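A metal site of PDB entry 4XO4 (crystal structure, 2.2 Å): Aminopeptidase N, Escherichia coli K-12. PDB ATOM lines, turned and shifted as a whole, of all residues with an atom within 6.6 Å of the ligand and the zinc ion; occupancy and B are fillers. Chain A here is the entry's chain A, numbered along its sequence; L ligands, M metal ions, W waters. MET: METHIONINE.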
ATOM      1  N   GLN A 119       6.278 -12.227 -22.330  1.00  0.00           N
ATOM      2  CA  GLN A 119       6.628 -13.581 -22.789  1.00  0.00           C
ATOM      3  C   GLN A 119       7.303 -13.439 -24.157  1.00  0.00           C
ATOM      4  O   GLN A 119       6.651 -12.965 -25.106  1.00  0.00           O
ATOM      5  CB  GLN A 119       5.381 -14.509 -22.884  1.00  0.00           C
ATOM      6  CG  GLN A 119       5.670 -15.883 -23.525  1.00  0.00           C
ATOM      7  CD  GLN A 119       6.737 -16.635 -22.737  1.00  0.00           C
ATOM      8  OE1 GLN A 119       6.823 -16.512 -21.523  1.00  0.00           O
ATOM      9  NE2 GLN A 119       7.561 -17.413 -23.413  1.00  0.00           N
ATOM     10  N   CYS A 120       8.586 -13.755 -24.240  1.00  0.00           N
ATOM     11  CA  CYS A 120       9.393 -13.583 -25.415  1.00  0.00           C
ATOM     12  C   CYS A 120       9.702 -14.854 -26.161  1.00  0.00           C
ATOM     13  O   CYS A 120       9.994 -14.796 -27.364  1.00  0.00           O
ATOM     14  CB  CYS A 120      10.679 -12.845 -25.095  1.00  0.00           C
ATOM     15  SG  CYS A 120      10.300 -11.115 -24.560  1.00  0.00           S
ATOM     16  N   GLU A 121       9.615 -16.000 -25.541  1.00  0.00           N
ATOM     17  CA  GLU A 121       9.901 -17.265 -26.280  1.00  0.00           C
ATOM     18  C   GLU A 121       8.656 -17.634 -27.097  1.00  0.00           C
ATOM     19  O   GLU A 121       7.601 -17.615 -26.555  1.00  0.00           O
ATOM     20  CB  GLU A 121      10.264 -18.445 -25.390  1.00  0.00           C
ATOM     21  CG  GLU A 121      10.810 -19.631 -26.243  1.00  0.00           C
ATOM     22  CD  GLU A 121      11.238 -20.883 -25.463  1.00  0.00           C
ATOM     23  OE1 GLU A 121      11.312 -20.823 -24.259  1.00  0.00           O
ATOM     24  OE2 GLU A 121      11.660 -21.909 -26.047  1.00  0.00           O
ATOM     25  N   ALA A 122       8.751 -18.010 -28.366  1.00  0.00           N
ATOM     26  CA  ALA A 122      10.018 -18.097 -29.150  1.00  0.00           C
ATOM     27  C   ALA A 122      10.378 -16.755 -29.804  1.00  0.00           C
ATOM     28  O   ALA A 122      11.548 -16.356 -29.760  1.00  0.00           O
ATOM     29  CB  ALA A 122       9.901 -19.188 -30.215  1.00  0.00           C
ATOM     30  N   TYR A 185      14.998 -14.144 -26.572  1.00  0.00           N
ATOM     31  CA  TYR A 185      13.843 -14.894 -25.982  1.00  0.00           C
ATOM     32  C   TYR A 185      13.848 -15.032 -24.466  1.00  0.00           C
ATOM     33  O   TYR A 185      12.856 -15.391 -23.863  1.00  0.00           O
ATOM     34  CB  TYR A 185      13.651 -16.260 -26.619  1.00  0.00           C
ATOM     35  CG  TYR A 185      14.579 -17.380 -26.206  1.00  0.00           C
ATOM     36  CD1 TYR A 185      14.242 -18.190 -25.150  1.00  0.00           C
ATOM     37  CD2 TYR A 185      15.751 -17.679 -26.913  1.00  0.00           C
ATOM     38  CE1 TYR A 185      15.016 -19.245 -24.803  1.00  0.00           C
ATOM     39  CE2 TYR A 185      16.576 -18.742 -26.512  1.00  0.00           C
ATOM     40  CZ  TYR A 185      16.176 -19.513 -25.483  1.00  0.00           C
ATOM     41  OH  TYR A 185      16.911 -20.541 -25.021  1.00  0.00           O
ATOM     42  N   PHE A 258      -1.255 -16.550 -18.721  1.00  0.00           N
ATOM     43  CA  PHE A 258      -0.015 -17.077 -19.249  1.00  0.00           C
ATOM     44  C   PHE A 258      -0.426 -18.212 -20.168  1.00  0.00           C
ATOM     45  O   PHE A 258      -1.237 -19.073 -19.776  1.00  0.00           O
ATOM     46  CB  PHE A 258       0.874 -17.586 -18.087  1.00  0.00           C
ATOM     47  CG  PHE A 258       2.298 -17.735 -18.482  1.00  0.00           C
ATOM     48  CD1 PHE A 258       3.061 -16.627 -18.678  1.00  0.00           C
ATOM     49  CD2 PHE A 258       2.841 -18.990 -18.734  1.00  0.00           C
ATOM     50  CE1 PHE A 258       4.390 -16.714 -19.081  1.00  0.00           C
ATOM     51  CE2 PHE A 258       4.156 -19.114 -19.183  1.00  0.00           C
ATOM     52  CZ  PHE A 258       4.942 -17.973 -19.342  1.00  0.00           C
ATOM     53  N   MET A 260       1.506 -20.694 -21.673  1.00  0.00           N
ATOM     54  CA  MET A 260       2.119 -21.986 -21.412  1.00  0.00           C
ATOM     55  C   MET A 260       2.194 -22.289 -19.913  1.00  0.00           C
ATOM     56  O   MET A 260       1.277 -21.883 -19.163  1.00  0.00           O
ATOM     57  CB  MET A 260       3.424 -22.024 -22.215  1.00  0.00           C
ATOM     58  CG  MET A 260       3.035 -22.318 -23.686  1.00  0.00           C
ATOM     59  SD  MET A 260       4.055 -21.557 -24.929  1.00  0.00           S
ATOM     60  CE  MET A 260       3.950 -19.770 -24.638  1.00  0.00           C
ATOM     61  N   GLY A 261       3.166 -23.060 -19.466  1.00  0.00           N
ATOM     62  CA  GLY A 261       3.251 -23.404 -18.083  1.00  0.00           C
ATOM     63  C   GLY A 261       4.144 -22.405 -17.365  1.00  0.00           C
ATOM     64  O   GLY A 261       3.788 -21.892 -16.329  1.00  0.00           O
ATOM     65  N   ALA A 262       5.342 -22.226 -17.889  1.00  0.00           N
ATOM     66  CA  ALA A 262       6.349 -21.392 -17.219  1.00  0.00           C
ATOM     67  C   ALA A 262       7.495 -21.082 -18.148  1.00  0.00           C
ATOM     68  O   ALA A 262       7.611 -21.679 -19.184  1.00  0.00           O
ATOM     69  CB  ALA A 262       6.834 -22.096 -15.992  1.00  0.00           C
ATOM     70  N   MET A 263       8.376 -20.160 -17.776  1.00  0.00           N
ATOM     71  CA  MET A 263       9.389 -19.648 -18.683  1.00  0.00           C
ATOM     72  C   MET A 263      10.690 -19.360 -17.949  1.00  0.00           C
ATOM     73  O   MET A 263      10.678 -18.683 -16.917  1.00  0.00           O
ATOM     74  CB  MET A 263       8.857 -18.426 -19.402  1.00  0.00           C
ATOM     75  CG  MET A 263       9.836 -17.805 -20.406  1.00  0.00           C
ATOM     76  SD  MET A 263      10.273 -19.005 -21.720  1.00  0.00           S
ATOM     77  CE  MET A 263      11.954 -18.519 -21.988  1.00  0.00           C
ATOM     78  N   GLU A 264      11.784 -19.899 -18.477  1.00  0.00           N
ATOM     79  CA  GLU A 264      13.092 -19.884 -17.839  1.00  0.00           C
ATOM     80  C   GLU A 264      13.912 -18.602 -18.057  1.00  0.00           C
ATOM     81  O   GLU A 264      15.157 -18.632 -18.059  1.00  0.00           O
ATOM     82  CB  GLU A 264      13.932 -21.074 -18.337  1.00  0.00           C
ATOM     83  CG  GLU A 264      14.437 -21.002 -19.812  1.00  0.00           C
ATOM     84  CD  GLU A 264      13.465 -21.601 -20.846  1.00  0.00           C
ATOM     85  OE1 GLU A 264      12.270 -21.700 -20.524  1.00  0.00           O
ATOM     86  OE2 GLU A 264      13.839 -21.998 -22.005  1.00  0.00           O
ATOM     87  N   VAL A 294       7.721 -28.569 -12.558  1.00  0.00           N
ATOM     88  CA  VAL A 294       7.830 -27.369 -13.371  1.00  0.00           C
ATOM     89  C   VAL A 294       8.852 -26.394 -12.808  1.00  0.00           C
ATOM     90  O   VAL A 294       9.624 -25.795 -13.593  1.00  0.00           O
ATOM     91  CB  VAL A 294       6.458 -26.726 -13.627  1.00  0.00           C
ATOM     92  CG1 VAL A 294       6.572 -25.426 -14.455  1.00  0.00           C
ATOM     93  CG2 VAL A 294       5.584 -27.747 -14.400  1.00  0.00           C
ATOM     94  N   HIS A 297      12.037 -27.976 -13.762  1.00  0.00           N
ATOM     95  CA  HIS A 297      12.219 -27.832 -15.206  1.00  0.00           C
ATOM     96  C   HIS A 297      12.813 -26.440 -15.538  1.00  0.00           C
ATOM     97  O   HIS A 297      13.850 -26.349 -16.182  1.00  0.00           O
ATOM     98  CB  HIS A 297      10.841 -28.015 -15.920  1.00  0.00           C
ATOM     99  CG  HIS A 297      10.933 -27.939 -17.406  1.00  0.00           C
ATOM    100  ND1 HIS A 297      11.154 -29.045 -18.183  1.00  0.00           N
ATOM    101  CD2 HIS A 297      10.940 -26.884 -18.244  1.00  0.00           C
ATOM    102  CE1 HIS A 297      11.248 -28.679 -19.448  1.00  0.00           C
ATOM    103  NE2 HIS A 297      11.148 -27.374 -19.506  1.00  0.00           N
ATOM    104  N   GLU A 298      12.177 -25.373 -15.085  1.00  0.00           N
ATOM    105  CA  GLU A 298      12.673 -24.042 -15.428  1.00  0.00           C
ATOM    106  C   GLU A 298      14.026 -23.785 -14.765  1.00  0.00           C
ATOM    107  O   GLU A 298      14.901 -23.234 -15.387  1.00  0.00           O
ATOM    108  CB  GLU A 298      11.695 -22.984 -15.100  1.00  0.00           C
ATOM    109  CG  GLU A 298      10.291 -23.227 -15.602  1.00  0.00           C
ATOM    110  CD  GLU A 298      10.167 -23.469 -17.095  1.00  0.00           C
ATOM    111  OE1 GLU A 298      11.066 -23.027 -17.828  1.00  0.00           O
ATOM    112  OE2 GLU A 298       9.161 -24.123 -17.522  1.00  0.00           O
ATOM    113  N   HIS A 301      16.764 -25.483 -16.855  1.00  0.00           N
ATOM    114  CA  HIS A 301      17.083 -24.711 -18.065  1.00  0.00           C
ATOM    115  C   HIS A 301      18.221 -23.697 -17.878  1.00  0.00           C
ATOM    116  O   HIS A 301      18.773 -23.182 -18.842  1.00  0.00           O
ATOM    117  CB  HIS A 301      15.885 -23.902 -18.529  1.00  0.00           C
ATOM    118  CG  HIS A 301      15.014 -24.573 -19.524  1.00  0.00           C
ATOM    119  ND1 HIS A 301      15.500 -25.194 -20.653  1.00  0.00           N
ATOM    120  CD2 HIS A 301      13.670 -24.699 -19.560  1.00  0.00           C
ATOM    121  CE1 HIS A 301      14.466 -25.619 -21.365  1.00  0.00           C
ATOM    122  NE2 HIS A 301      13.363 -25.337 -20.709  1.00  0.00           N
ATOM    123  N   LEU A 316      15.035 -26.809 -30.955  1.00  0.00           N
ATOM    124  CA  LEU A 316      14.330 -26.676 -29.700  1.00  0.00           C
ATOM    125  C   LEU A 316      14.516 -27.885 -28.747  1.00  0.00           C
ATOM    126  O   LEU A 316      14.704 -27.695 -27.541  1.00  0.00           O
ATOM    127  CB  LEU A 316      12.825 -26.467 -29.920  1.00  0.00           C
ATOM    128  CG  LEU A 316      11.912 -26.252 -28.707  1.00  0.00           C
ATOM    129  CD1 LEU A 316      12.329 -25.083 -27.830  1.00  0.00           C
ATOM    130  CD2 LEU A 316      10.497 -25.993 -29.135  1.00  0.00           C
ATOM    131  N   LYS A 319      17.348 -28.098 -25.961  1.00  0.00           N
ATOM    132  CA  LYS A 319      17.021 -27.693 -24.627  1.00  0.00           C
ATOM    133  C   LYS A 319      15.797 -28.371 -24.025  1.00  0.00           C
ATOM    134  O   LYS A 319      15.822 -28.694 -22.844  1.00  0.00           O
ATOM    135  CB  LYS A 319      16.910 -26.188 -24.534  1.00  0.00           C
ATOM    136  CG  LYS A 319      15.690 -25.544 -25.115  1.00  0.00           C
ATOM    137  CD  LYS A 319      15.831 -24.029 -24.943  1.00  0.00           C
ATOM    138  CE  LYS A 319      14.650 -23.151 -25.393  1.00  0.00           C
ATOM    139  NZ  LYS A 319      13.456 -23.164 -24.522  1.00  0.00           N
ATOM    140  N   GLU A 320      14.722 -28.615 -24.805  1.00  0.00           N
ATOM    141  CA  GLU A 320      13.548 -29.192 -24.225  1.00  0.00           C
ATOM    142  C   GLU A 320      13.659 -30.699 -23.922  1.00  0.00           C
ATOM    143  O   GLU A 320      13.179 -31.124 -22.892  1.00  0.00           O
ATOM    144  CB  GLU A 320      12.272 -28.873 -25.029  1.00  0.00           C
ATOM    145  CG  GLU A 320      11.939 -27.373 -25.136  1.00  0.00           C
ATOM    146  CD  GLU A 320      11.888 -26.689 -23.790  1.00  0.00           C
ATOM    147  OE1 GLU A 320      11.797 -27.435 -22.791  1.00  0.00           O
ATOM    148  OE2 GLU A 320      12.034 -25.449 -23.736  1.00  0.00           O
ATOM    149  N   THR A 323      16.094 -30.970 -20.989  1.00  0.00           N
ATOM    150  CA  THR A 323      15.533 -30.394 -19.776  1.00  0.00           C
ATOM    151  C   THR A 323      14.350 -31.221 -19.247  1.00  0.00           C
ATOM    152  O   THR A 323      14.182 -31.355 -18.043  1.00  0.00           O
ATOM    153  CB  THR A 323      15.205 -28.900 -19.937  1.00  0.00           C
ATOM    154  OG1 THR A 323      16.388 -28.173 -20.321  1.00  0.00           O
ATOM    155  CG2 THR A 323      14.721 -28.311 -18.645  1.00  0.00           C
ATOM    156  N   VAL A 324      13.517 -31.768 -20.112  1.00  0.00           N
ATOM    157  CA  VAL A 324      12.498 -32.713 -19.671  1.00  0.00           C
ATOM    158  C   VAL A 324      13.099 -33.991 -19.045  1.00  0.00           C
ATOM    159  O   VAL A 324      12.650 -34.429 -17.968  1.00  0.00           O
ATOM    160  CB  VAL A 324      11.525 -33.092 -20.804  1.00  0.00           C
ATOM    161  CG1 VAL A 324      10.595 -34.239 -20.385  1.00  0.00           C
ATOM    162  CG2 VAL A 324      10.669 -31.894 -21.187  1.00  0.00           C
ATOM    163  N   ASN A 373       5.419 -21.441 -32.519  1.00  0.00           N
ATOM    164  CA  ASN A 373       4.643 -21.802 -31.356  1.00  0.00           C
ATOM    165  C   ASN A 373       3.866 -23.097 -31.538  1.00  0.00           C
ATOM    166  O   ASN A 373       3.420 -23.691 -30.557  1.00  0.00           O
ATOM    167  CB  ASN A 373       3.669 -20.675 -30.965  1.00  0.00           C
ATOM    168  CG  ASN A 373       4.377 -19.488 -30.350  1.00  0.00           C
ATOM    169  OD1 ASN A 373       5.483 -19.601 -29.769  1.00  0.00           O
ATOM    170  ND2 ASN A 373       3.807 -18.292 -30.615  1.00  0.00           N
ATOM    171  N   TYR A 376       5.979 -26.560 -29.819  1.00  0.00           N
ATOM    172  CA  TYR A 376       6.106 -26.853 -28.411  1.00  0.00           C
ATOM    173  C   TYR A 376       5.266 -28.076 -28.118  1.00  0.00           C
ATOM    174  O   TYR A 376       4.207 -27.981 -27.502  1.00  0.00           O
ATOM    175  CB  TYR A 376       5.737 -25.613 -27.550  1.00  0.00           C
ATOM    176  CG  TYR A 376       6.861 -24.586 -27.695  1.00  0.00           C
ATOM    177  CD1 TYR A 376       6.962 -23.771 -28.833  1.00  0.00           C
ATOM    178  CD2 TYR A 376       7.882 -24.520 -26.754  1.00  0.00           C
ATOM    179  CE1 TYR A 376       8.014 -22.913 -29.045  1.00  0.00           C
ATOM    180  CE2 TYR A 376       8.968 -23.647 -26.921  1.00  0.00           C
ATOM    181  CZ  TYR A 376       9.014 -22.842 -28.044  1.00  0.00           C
ATOM    182  OH  TYR A 376      10.064 -22.028 -28.235  1.00  0.00           O
ATOM    183  N   TYR A 381       9.196 -32.373 -26.765  1.00  0.00           N
ATOM    184  CA  TYR A 381       9.420 -32.483 -25.334  1.00  0.00           C
ATOM    185  C   TYR A 381       9.586 -33.976 -24.830  1.00  0.00           C
ATOM    186  O   TYR A 381      10.613 -34.378 -24.233  1.00  0.00           O
ATOM    187  CB  TYR A 381       8.258 -31.815 -24.531  1.00  0.00           C
ATOM    188  CG  TYR A 381       8.353 -30.326 -24.421  1.00  0.00           C
ATOM    189  CD1 TYR A 381       8.235 -29.495 -25.548  1.00  0.00           C
ATOM    190  CD2 TYR A 381       8.536 -29.697 -23.158  1.00  0.00           C
ATOM    191  CE1 TYR A 381       8.338 -28.094 -25.439  1.00  0.00           C
ATOM    192  CE2 TYR A 381       8.678 -28.302 -23.030  1.00  0.00           C
ATOM    193  CZ  TYR A 381       8.548 -27.483 -24.142  1.00  0.00           C
ATOM    194  OH  TYR A 381       8.710 -26.069 -24.003  1.00  0.00           O
ATOM    195  N   GLN A 821      -2.432 -18.796 -30.063  1.00  0.00           N
ATOM    196  CA  GLN A 821      -1.683 -19.910 -29.481  1.00  0.00           C
ATOM    197  C   GLN A 821      -2.615 -20.842 -28.755  1.00  0.00           C
ATOM    198  O   GLN A 821      -2.493 -22.038 -28.876  1.00  0.00           O
ATOM    199  CB  GLN A 821      -0.689 -19.481 -28.446  1.00  0.00           C
ATOM    200  CG  GLN A 821       0.534 -18.939 -29.033  1.00  0.00           C
ATOM    201  CD  GLN A 821       1.648 -18.781 -27.956  1.00  0.00           C
ATOM    202  OE1 GLN A 821       2.073 -19.762 -27.251  1.00  0.00           O
ATOM    203  NE2 GLN A 821       2.143 -17.577 -27.853  1.00  0.00           N
HETATM  204  N   MET L   1      10.723 -23.289 -22.716  1.00  0.00           N
HETATM  205  CA  MET L   1       9.809 -23.195 -21.516  1.00  0.00           C
HETATM  206  C   MET L   1       9.269 -24.532 -20.993  1.00  0.00           C
HETATM  207  O   MET L   1       9.884 -25.486 -21.377  1.00  0.00           O
HETATM  208  CB  MET L   1       8.654 -22.272 -21.840  1.00  0.00           C
HETATM  209  CG  MET L   1       7.736 -22.710 -22.954  1.00  0.00           C
HETATM  210  SD  MET L   1       7.070 -21.116 -23.497  1.00  0.00           S
HETATM  211  CE  MET L   1       7.746 -20.962 -25.140  1.00  0.00           C
HETATM  212  OXT MET L   1       8.251 -24.662 -20.291  1.00  0.00           O
HETATM  213 ZN    ZN M   1      11.477 -26.196 -21.157  1.00  0.00          ZN
HETATM  214  O   HOH W   1       6.376 -26.835 -18.789  1.00  0.00           O
HETATM  215  O   HOH W   2       5.731 -24.378 -20.478  1.00  0.00           O
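OE1 of Glu 264 is in salt-bridge range of N of the ligand, at 3.1 Å.
O of the ligand sits close to OH of Tyr 381, at 2.9 Å.
The side-chain carboxylate (OE2) of Glu 298 sits close to an oxygen (OXT) of the ligand, 3.0 Å away.
NE2 of Gln 119 lies close to SD of the ligand (3.7 Å).
The side-chain amino group (NZ) of Lys 319 lies close to a nitrogen (N) of the ligand (3.3 Å).
The side-chain carboxylate of Glu 121 lies within salt-bridge range of a nitrogen (N) of the ligand (3.0 Å).
The side-chain carboxylate (OE2) of Glu 320 is in salt-bridge range of the side-chain amino group (NZ) of Lys 319.
SD of Met 263 lies within hydrogen-bond range of NE2 of Gln 119 (3.6 Å).
A ring nitrogen (ND1) of His 301 is in hydrogen-bond range of the side-chain hydroxyl (OG1) of Thr 323 (3.1 Å).
OE2 of Glu 320 lies close to OH of Tyr 381, 3.4 Å away.
NZ of Lys 319 lies within salt-bridge range of OE2 of Glu 121 (2.7 Å).
The side-chain carboxylate of Glu 298 sits at hydrogen-bond distance from the backbone NH of Glu 264, 3.3 Å away.
OE1 of Gln 821 sits close to SD of Met 260, at 3.5 Å.
The backbone carbonyl oxygen (O) of Glu 121 lies within hydrogen-bond range of the side-chain amide nitrogen (NE2) of Gln 119, 3.1 Å away.
SD of Met 260 sits close to SD of the ligand.
OXT of the ligand lies close to O of Ala 262, 3.2 Å away.
Merely in contact with the ligand: Tyr 376 and Met 263.
Of the 24 residues printed, 13 come within 4 Å of the ligand.
Along chain A the residues within 4 Å of the ligand span positions 119 to 381.
Merely in contact with the zinc ion: Tyr 381 (3.97 Å).
O of the ligand binds the zinc ion, at 1.8 Å.
NE2 of His 297 binds the zinc ion.
The zinc ion is bound by the side-chain carboxylate (OE1) of Glu 320.
A ring nitrogen (NE2) of His 301 is bound to the zinc ion (2.1 Å).
Slightly farther from the zinc ion lies OE2 of Glu 320 (2.7 Å).
Water W2 lies within hydrogen-bond range of OXT of the ligand (2.5 Å), N of Gly 261 (3.1 Å) and N of Ala 262 (3.4 Å).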
